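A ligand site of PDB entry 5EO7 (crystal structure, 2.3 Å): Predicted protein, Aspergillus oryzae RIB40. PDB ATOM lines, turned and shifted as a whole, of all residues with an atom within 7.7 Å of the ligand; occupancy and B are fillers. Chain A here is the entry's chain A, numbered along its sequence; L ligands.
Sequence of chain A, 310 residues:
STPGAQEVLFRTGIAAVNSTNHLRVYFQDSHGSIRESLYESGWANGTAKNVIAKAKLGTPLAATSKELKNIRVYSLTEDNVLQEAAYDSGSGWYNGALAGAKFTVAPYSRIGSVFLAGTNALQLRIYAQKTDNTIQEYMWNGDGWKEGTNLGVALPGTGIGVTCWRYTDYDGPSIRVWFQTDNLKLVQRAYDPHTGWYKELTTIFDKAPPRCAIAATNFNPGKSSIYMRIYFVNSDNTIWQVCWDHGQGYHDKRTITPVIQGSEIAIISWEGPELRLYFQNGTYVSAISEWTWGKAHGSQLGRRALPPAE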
ATOM      1  N   ASN A  70     -29.489  -9.982  -7.180  1.00  0.00           N
ATOM      2  CA  ASN A  70     -29.090  -9.548  -5.840  1.00  0.00           C
ATOM      3  C   ASN A  70     -28.384 -10.684  -5.118  1.00  0.00           C
ATOM      4  O   ASN A  70     -28.913 -11.791  -5.026  1.00  0.00           O
ATOM      5  CB  ASN A  70     -30.314  -9.085  -5.044  1.00  0.00           C
ATOM      6  CG  ASN A  70     -31.186  -8.135  -5.832  1.00  0.00           C
ATOM      7  OD1 ASN A  70     -32.217  -8.533  -6.382  1.00  0.00           O
ATOM      8  ND2 ASN A  70     -30.783  -6.871  -5.898  1.00  0.00           N
ATOM      9  N   ILE A  71     -27.191 -10.397  -4.608  1.00  0.00           N
ATOM     10  CA  ILE A  71     -26.417 -11.384  -3.873  1.00  0.00           C
ATOM     11  C   ILE A  71     -25.940 -10.780  -2.563  1.00  0.00           C
ATOM     12  O   ILE A  71     -25.528  -9.630  -2.506  1.00  0.00           O
ATOM     13  CB  ILE A  71     -25.179 -11.862  -4.659  1.00  0.00           C
ATOM     14  CG1 ILE A  71     -25.597 -12.338  -6.058  1.00  0.00           C
ATOM     15  CG2 ILE A  71     -24.462 -12.972  -3.906  1.00  0.00           C
ATOM     16  CD1 ILE A  71     -24.433 -12.605  -6.980  1.00  0.00           C
ATOM     17  N   ARG A  72     -26.006 -11.579  -1.504  1.00  0.00           N
ATOM     18  CA  ARG A  72     -25.503 -11.174  -0.199  1.00  0.00           C
ATOM     19  C   ARG A  72     -24.608 -12.274   0.358  1.00  0.00           C
ATOM     20  O   ARG A  72     -24.970 -13.438   0.350  1.00  0.00           O
ATOM     21  CB  ARG A  72     -26.669 -10.879   0.755  1.00  0.00           C
ATOM     22  CG  ARG A  72     -27.643  -9.817   0.243  1.00  0.00           C
ATOM     23  CD  ARG A  72     -27.009  -8.438   0.194  1.00  0.00           C
ATOM     24  NE  ARG A  72     -27.974  -7.409  -0.201  1.00  0.00           N
ATOM     25  CZ  ARG A  72     -28.262  -7.084  -1.450  1.00  0.00           C
ATOM     26  NH1 ARG A  72     -27.659  -7.699  -2.468  1.00  0.00           N
ATOM     27  NH2 ARG A  72     -29.155  -6.144  -1.694  1.00  0.00           N
ATOM     28  N   TYR A  74     -22.216 -13.216   3.755  1.00  0.00           N
ATOM     29  CA  TYR A  74     -22.012 -12.859   5.148  1.00  0.00           C
ATOM     30  C   TYR A  74     -20.777 -13.501   5.766  1.00  0.00           C
ATOM     31  O   TYR A  74     -20.451 -14.650   5.475  1.00  0.00           O
ATOM     32  CB  TYR A  74     -23.259 -13.232   5.966  1.00  0.00           C
ATOM     33  CG  TYR A  74     -24.505 -12.573   5.424  1.00  0.00           C
ATOM     34  CD1 TYR A  74     -24.880 -11.311   5.844  1.00  0.00           C
ATOM     35  CD2 TYR A  74     -25.279 -13.217   4.471  1.00  0.00           C
ATOM     36  CE1 TYR A  74     -26.003 -10.702   5.341  1.00  0.00           C
ATOM     37  CE2 TYR A  74     -26.413 -12.615   3.961  1.00  0.00           C
ATOM     38  CZ  TYR A  74     -26.770 -11.359   4.406  1.00  0.00           C
ATOM     39  OH  TYR A  74     -27.901 -10.747   3.897  1.00  0.00           O
ATOM     40  N   GLU A  84     -21.660  -7.882   5.904  1.00  0.00           N
ATOM     41  CA  GLU A  84     -22.363  -8.274   4.693  1.00  0.00           C
ATOM     42  C   GLU A  84     -21.743  -7.626   3.465  1.00  0.00           C
ATOM     43  O   GLU A  84     -21.645  -6.399   3.374  1.00  0.00           O
ATOM     44  CB  GLU A  84     -23.842  -7.887   4.809  1.00  0.00           C
ATOM     45  CG  GLU A  84     -24.640  -7.936   3.524  1.00  0.00           C
ATOM     46  CD  GLU A  84     -26.044  -7.375   3.706  1.00  0.00           C
ATOM     47  OE1 GLU A  84     -27.024  -8.148   3.602  1.00  0.00           O
ATOM     48  OE2 GLU A  84     -26.176  -6.160   3.956  1.00  0.00           O
ATOM     49  N   ALA A  85     -21.323  -8.465   2.516  1.00  0.00           N
ATOM     50  CA  ALA A  85     -20.943  -8.005   1.184  1.00  0.00           C
ATOM     51  C   ALA A  85     -22.171  -8.130   0.288  1.00  0.00           C
ATOM     52  O   ALA A  85     -22.788  -9.186   0.220  1.00  0.00           O
ATOM     53  CB  ALA A  85     -19.789  -8.823   0.640  1.00  0.00           C
ATOM     54  N   ALA A  86     -22.506  -7.043  -0.395  1.00  0.00           N
ATOM     55  CA  ALA A  86     -23.737  -6.982  -1.182  1.00  0.00           C
ATOM     56  C   ALA A  86     -23.457  -6.715  -2.657  1.00  0.00           C
ATOM     57  O   ALA A  86     -22.666  -5.836  -2.993  1.00  0.00           O
ATOM     58  CB  ALA A  86     -24.657  -5.906  -0.627  1.00  0.00           C
ATOM     59  N   TYR A  87     -24.116  -7.492  -3.523  1.00  0.00           N
ATOM     60  CA  TYR A  87     -24.099  -7.237  -4.948  1.00  0.00           C
ATOM     61  C   TYR A  87     -25.504  -6.959  -5.442  1.00  0.00           C
ATOM     62  O   TYR A  87     -26.423  -7.733  -5.188  1.00  0.00           O
ATOM     63  CB  TYR A  87     -23.514  -8.420  -5.726  1.00  0.00           C
ATOM     64  CG  TYR A  87     -23.522  -8.215  -7.224  1.00  0.00           C
ATOM     65  CD1 TYR A  87     -24.635  -8.529  -7.981  1.00  0.00           C
ATOM     66  CD2 TYR A  87     -22.401  -7.706  -7.883  1.00  0.00           C
ATOM     67  CE1 TYR A  87     -24.650  -8.343  -9.350  1.00  0.00           C
ATOM     68  CE2 TYR A  87     -22.415  -7.510  -9.251  1.00  0.00           C
ATOM     69  CZ  TYR A  87     -23.539  -7.835  -9.978  1.00  0.00           C
ATOM     70  OH  TYR A  87     -23.546  -7.651 -11.342  1.00  0.00           O
ATOM     71  N   ASP A  88     -25.663  -5.844  -6.152  1.00  0.00           N
ATOM     72  CA  ASP A  88     -26.901  -5.553  -6.860  1.00  0.00           C
ATOM     73  C   ASP A  88     -26.601  -5.300  -8.333  1.00  0.00           C
ATOM     74  O   ASP A  88     -25.693  -4.538  -8.666  1.00  0.00           O
ATOM     75  CB  ASP A  88     -27.611  -4.339  -6.266  1.00  0.00           C
ATOM     76  CG  ASP A  88     -28.174  -4.611  -4.888  1.00  0.00           C
ATOM     77  OD1 ASP A  88     -28.619  -5.749  -4.627  1.00  0.00           O
ATOM     78  OD2 ASP A  88     -28.190  -3.671  -4.069  1.00  0.00           O
ATOM     79  N   TYR A  94     -20.688  -3.840  -2.946  1.00  0.00           N
ATOM     80  CA  TYR A  94     -20.526  -2.809  -1.937  1.00  0.00           C
ATOM     81  C   TYR A  94     -20.722  -3.374  -0.532  1.00  0.00           C
ATOM     82  O   TYR A  94     -21.250  -4.467  -0.367  1.00  0.00           O
ATOM     83  CB  TYR A  94     -21.509  -1.656  -2.170  1.00  0.00           C
ATOM     84  CG  TYR A  94     -22.950  -2.079  -2.126  1.00  0.00           C
ATOM     85  CD1 TYR A  94     -23.594  -2.540  -3.268  1.00  0.00           C
ATOM     86  CD2 TYR A  94     -23.679  -2.026  -0.941  1.00  0.00           C
ATOM     87  CE1 TYR A  94     -24.923  -2.936  -3.232  1.00  0.00           C
ATOM     88  CE2 TYR A  94     -24.998  -2.413  -0.899  1.00  0.00           C
ATOM     89  CZ  TYR A  94     -25.612  -2.870  -2.046  1.00  0.00           C
ATOM     90  OH  TYR A  94     -26.939  -3.256  -2.010  1.00  0.00           O
ATOM     91  N   ASN A  95     -20.297  -2.622   0.479  1.00  0.00           N
ATOM     92  CA  ASN A  95     -20.521  -3.006   1.866  1.00  0.00           C
ATOM     93  C   ASN A  95     -21.987  -2.835   2.222  1.00  0.00           C
ATOM     94  O   ASN A  95     -22.557  -1.762   2.046  1.00  0.00           O
ATOM     95  CB  ASN A  95     -19.660  -2.163   2.806  1.00  0.00           C
ATOM     96  CG  ASN A  95     -18.175  -2.402   2.613  1.00  0.00           C
ATOM     97  OD1 ASN A  95     -17.751  -3.507   2.289  1.00  0.00           O
ATOM     98  ND2 ASN A  95     -17.382  -1.351   2.802  1.00  0.00           N
ATOM     99  N   GLY A  96     -22.594  -3.908   2.720  1.00  0.00           N
ATOM    100  CA  GLY A  96     -23.979  -3.873   3.140  1.00  0.00           C
ATOM    101  C   GLY A  96     -24.119  -3.195   4.484  1.00  0.00           C
ATOM    102  O   GLY A  96     -23.129  -2.974   5.186  1.00  0.00           O
ATOM    103  N   ALA A  97     -25.357  -2.890   4.868  1.00  0.00           N
ATOM    104  CA  ALA A  97     -25.622  -2.125   6.085  1.00  0.00           C
ATOM    105  C   ALA A  97     -25.550  -2.960   7.361  1.00  0.00           C
ATOM    106  O   ALA A  97     -25.653  -2.414   8.460  1.00  0.00           O
ATOM    107  CB  ALA A  97     -26.985  -1.477   5.973  1.00  0.00           C
ATOM    108  N   LEU A  98     -25.387  -4.273   7.224  1.00  0.00           N
ATOM    109  CA  LEU A  98     -25.465  -5.171   8.390  1.00  0.00           C
ATOM    110  C   LEU A  98     -24.467  -4.810   9.489  1.00  0.00           C
ATOM    111  O   LEU A  98     -24.842  -4.726  10.660  1.00  0.00           O
ATOM    112  CB  LEU A  98     -25.251  -6.625   7.968  1.00  0.00           C
ATOM    113  CG  LEU A  98     -25.290  -7.661   9.096  1.00  0.00           C
ATOM    114  CD1 LEU A  98     -26.637  -7.647   9.810  1.00  0.00           C
ATOM    115  CD2 LEU A  98     -25.001  -9.059   8.552  1.00  0.00           C
ATOM    116  N   ALA A  99     -23.212  -4.607   9.112  1.00  0.00           N
ATOM    117  CA  ALA A  99     -22.173  -4.297  10.097  1.00  0.00           C
ATOM    118  C   ALA A  99     -22.521  -3.051  10.900  1.00  0.00           C
ATOM    119  O   ALA A  99     -22.111  -2.901  12.046  1.00  0.00           O
ATOM    120  CB  ALA A  99     -20.836  -4.127   9.413  1.00  0.00           C
ATOM    121  N   PHE A 115     -32.846 -15.230   1.503  1.00  0.00           N
ATOM    122  CA  PHE A 115     -33.856 -14.299   1.046  1.00  0.00           C
ATOM    123  C   PHE A 115     -35.194 -14.982   1.238  1.00  0.00           C
ATOM    124  O   PHE A 115     -35.313 -16.188   1.010  1.00  0.00           O
ATOM    125  CB  PHE A 115     -33.648 -13.915  -0.425  1.00  0.00           C
ATOM    126  CG  PHE A 115     -32.733 -12.745  -0.632  1.00  0.00           C
ATOM    127  CD1 PHE A 115     -33.160 -11.450  -0.358  1.00  0.00           C
ATOM    128  CD2 PHE A 115     -31.449 -12.928  -1.124  1.00  0.00           C
ATOM    129  CE1 PHE A 115     -32.319 -10.379  -0.550  1.00  0.00           C
ATOM    130  CE2 PHE A 115     -30.608 -11.856  -1.316  1.00  0.00           C
ATOM    131  CZ  PHE A 115     -31.042 -10.571  -1.035  1.00  0.00           C
ATOM    132  N   ALA A 121     -40.043  -8.295  -3.239  1.00  0.00           N
ATOM    133  CA  ALA A 121     -39.397  -7.399  -2.292  1.00  0.00           C
ATOM    134  C   ALA A 121     -38.189  -8.097  -1.676  1.00  0.00           C
ATOM    135  O   ALA A 121     -38.161  -9.330  -1.572  1.00  0.00           O
ATOM    136  CB  ALA A 121     -40.362  -6.970  -1.219  1.00  0.00           C
ATOM    137  N   LEU A 122     -37.192  -7.311  -1.271  1.00  0.00           N
ATOM    138  CA  LEU A 122     -35.947  -7.864  -0.760  1.00  0.00           C
ATOM    139  C   LEU A 122     -35.976  -8.012   0.758  1.00  0.00           C
ATOM    140  O   LEU A 122     -35.650  -7.084   1.496  1.00  0.00           O
ATOM    141  CB  LEU A 122     -34.769  -6.968  -1.160  1.00  0.00           C
ATOM    142  CG  LEU A 122     -34.222  -7.160  -2.582  1.00  0.00           C
ATOM    143  CD1 LEU A 122     -35.271  -6.838  -3.636  1.00  0.00           C
ATOM    144  CD2 LEU A 122     -32.980  -6.313  -2.788  1.00  0.00           C
ATOM    145  N   GLN A 123     -36.383  -9.195   1.217  1.00  0.00           N
ATOM    146  CA  GLN A 123     -36.422  -9.517   2.630  1.00  0.00           C
ATOM    147  C   GLN A 123     -35.389 -10.586   2.966  1.00  0.00           C
ATOM    148  O   GLN A 123     -35.261 -11.578   2.251  1.00  0.00           O
ATOM    149  CB  GLN A 123     -37.814  -9.981   3.051  1.00  0.00           C
ATOM    150  CG  GLN A 123     -38.881  -8.919   2.887  1.00  0.00           C
ATOM    151  CD  GLN A 123     -40.235  -9.359   3.406  1.00  0.00           C
ATOM    152  OE1 GLN A 123     -41.070  -9.874   2.657  1.00  0.00           O
ATOM    153  NE2 GLN A 123     -40.474  -9.148   4.698  1.00  0.00           N
ATOM    154  N   LEU A 124     -34.641 -10.355   4.035  1.00  0.00           N
ATOM    155  CA  LEU A 124     -33.576 -11.264   4.456  1.00  0.00           C
ATOM    156  C   LEU A 124     -33.770 -11.760   5.882  1.00  0.00           C
ATOM    157  O   LEU A 124     -34.214 -11.013   6.759  1.00  0.00           O
ATOM    158  CB  LEU A 124     -32.214 -10.583   4.353  1.00  0.00           C
ATOM    159  CG  LEU A 124     -31.677 -10.344   2.947  1.00  0.00           C
ATOM    160  CD1 LEU A 124     -30.726  -9.157   2.945  1.00  0.00           C
ATOM    161  CD2 LEU A 124     -30.983 -11.591   2.417  1.00  0.00           C
ATOM    162  N   TRP A 140     -33.973  -8.247   7.790  1.00  0.00           N
ATOM    163  CA  TRP A 140     -34.095  -7.041   6.991  1.00  0.00           C
ATOM    164  C   TRP A 140     -35.431  -7.086   6.260  1.00  0.00           C
ATOM    165  O   TRP A 140     -35.741  -8.073   5.584  1.00  0.00           O
ATOM    166  CB  TRP A 140     -32.947  -6.919   5.987  1.00  0.00           C
ATOM    167  CG  TRP A 140     -33.112  -5.776   5.065  1.00  0.00           C
ATOM    168  CD1 TRP A 140     -33.866  -5.743   3.926  1.00  0.00           C
ATOM    169  CD2 TRP A 140     -32.524  -4.474   5.195  1.00  0.00           C
ATOM    170  NE1 TRP A 140     -33.780  -4.505   3.341  1.00  0.00           N
ATOM    171  CE2 TRP A 140     -32.964  -3.710   4.095  1.00  0.00           C
ATOM    172  CE3 TRP A 140     -31.664  -3.897   6.127  1.00  0.00           C
ATOM    173  CZ2 TRP A 140     -32.574  -2.393   3.908  1.00  0.00           C
ATOM    174  CZ3 TRP A 140     -31.274  -2.579   5.939  1.00  0.00           C
ATOM    175  CH2 TRP A 140     -31.733  -1.842   4.840  1.00  0.00           C
ATOM    176  N   ASN A 141     -36.229  -6.032   6.403  1.00  0.00           N
ATOM    177  CA  ASN A 141     -37.534  -5.967   5.759  1.00  0.00           C
ATOM    178  C   ASN A 141     -37.779  -4.640   5.038  1.00  0.00           C
ATOM    179  O   ASN A 141     -38.901  -4.345   4.627  1.00  0.00           O
ATOM    180  CB  ASN A 141     -38.633  -6.204   6.792  1.00  0.00           C
ATOM    181  CG  ASN A 141     -38.684  -7.646   7.268  1.00  0.00           C
ATOM    182  OD1 ASN A 141     -38.483  -8.577   6.490  1.00  0.00           O
ATOM    183  ND2 ASN A 141     -38.949  -7.839   8.554  1.00  0.00           N
ATOM    184  N   GLY A 142     -36.717  -3.851   4.869  1.00  0.00           N
ATOM    185  CA  GLY A 142     -36.795  -2.624   4.086  1.00  0.00           C
ATOM    186  C   GLY A 142     -36.137  -1.419   4.721  1.00  0.00           C
ATOM    187  O   GLY A 142     -35.484  -0.636   4.029  1.00  0.00           O
ATOM    188  N   GLY A 144     -33.817  -1.178   7.863  1.00  0.00           N
ATOM    189  CA  GLY A 144     -32.926  -1.431   8.974  1.00  0.00           C
ATOM    190  C   GLY A 144     -32.908  -2.867   9.461  1.00  0.00           C
ATOM    191  O   GLY A 144     -33.878  -3.607   9.302  1.00  0.00           O
ATOM    192  N   TRP A 145     -31.781  -3.250  10.063  1.00  0.00           N
ATOM    193  CA  TRP A 145     -31.612  -4.598  10.599  1.00  0.00           C
ATOM    194  C   TRP A 145     -32.136  -4.678  12.029  1.00  0.00           C
ATOM    195  O   TRP A 145     -31.830  -3.825  12.856  1.00  0.00           O
ATOM    196  CB  TRP A 145     -30.147  -5.008  10.548  1.00  0.00           C
ATOM    197  CG  TRP A 145     -29.671  -5.364   9.184  1.00  0.00           C
ATOM    198  CD1 TRP A 145     -29.051  -4.548   8.285  1.00  0.00           C
ATOM    199  CD2 TRP A 145     -29.796  -6.648   8.543  1.00  0.00           C
ATOM    200  NE1 TRP A 145     -28.774  -5.238   7.133  1.00  0.00           N
ATOM    201  CE2 TRP A 145     -29.229  -6.528   7.262  1.00  0.00           C
ATOM    202  CE3 TRP A 145     -30.341  -7.868   8.935  1.00  0.00           C
ATOM    203  CZ2 TRP A 145     -29.170  -7.594   6.371  1.00  0.00           C
ATOM    204  CZ3 TRP A 145     -30.283  -8.935   8.043  1.00  0.00           C
ATOM    205  CH2 TRP A 145     -29.707  -8.787   6.778  1.00  0.00           C
HETATM  206  C1  LIG L   1     -29.032  -3.544   0.796  1.00  0.00           C
HETATM  207  C2  LIG L   1     -28.111  -3.879   1.958  1.00  0.00           C
HETATM  208  C3  LIG L   1     -28.958  -4.326   3.176  1.00  0.00           C
HETATM  209  C4  LIG L   1     -29.788  -5.531   2.716  1.00  0.00           C
HETATM  210  C5  LIG L   1     -30.742  -5.120   1.576  1.00  0.00           C
HETATM  211  C6  LIG L   1     -31.591  -6.289   1.100  1.00  0.00           C
HETATM  212  O1  LIG L   1     -27.347  -2.786   2.453  1.00  0.00           O
HETATM  213  O2  LIG L   1     -28.122  -4.708   4.246  1.00  0.00           O
HETATM  214  O3  LIG L   1     -28.921  -6.601   2.343  1.00  0.00           O
HETATM  215  O4  LIG L   1     -30.002  -4.537   0.471  1.00  0.00           O
HETATM  216  C7  LIG L   1     -31.016  -1.663  -0.445  1.00  0.00           C
HETATM  217 SE1  LIG L   1     -29.983  -1.847   1.220  1.00  0.00          SE
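The side-chain hydroxyl (OH) of Tyr 94 lies within hydrogen-bond range of the side-chain carboxylate (OD2) of Asp 88 (2.4 Å). The side-chain hydroxyl of Tyr 74 is in hydrogen-bond range of the side-chain carboxylate of Glu 84 (2.8 Å). NH1 of Arg 72 sits at hydrogen-bond distance from O of Tyr 87. OE1 of Glu 84 lies within salt-bridge range of NE of Arg 72, 3.99 Å away. N of Tyr 94 is in hydrogen-bond range of O of Ala 86 (2.8 Å). The backbone carbonyl oxygen of Glu 84 is in hydrogen-bond range of the backbone NH of Gly 96 (2.7 Å). The backbone NH (N) of Ala 97 sits at hydrogen-bond distance from the side-chain carboxylate (OE2) of Glu 84 (3.5 Å). NH2 of Arg 72 is in salt-bridge range of OD1 of Asp 88 (3.0 Å).
NH2 of Arg 72 is in hydrogen-bond range of O4 of the ligand (2.8 Å). The indole nitrogen (NE1) of Trp 145 sits at hydrogen-bond distance from an oxygen (O2) of the ligand (3.0 Å). N of Ala 97 lies within hydrogen-bond range of O1 of the ligand (3.1 Å). An oxygen (O2) of the ligand lies within hydrogen-bond range of the side-chain carboxylate of Glu 84, at 2.4 Å.
Tyr 94 touches the ligand. Gly 96 touches the ligand (CA to O1, 3.6 Å). Leu 122 touches the ligand. CD1 of Leu 124 touches O3 of the ligand, at 3.2 Å. Trp 140 touches the ligand (NE1 to C5, 3.6 Å). Hydrophobic or aromatic side chains within 4 Å of the ligand: Ala 97, Leu 122, Leu 124, Trp 140 and Trp 145. Of the 25 residues printed, 9 come within 4 Å of the ligand.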
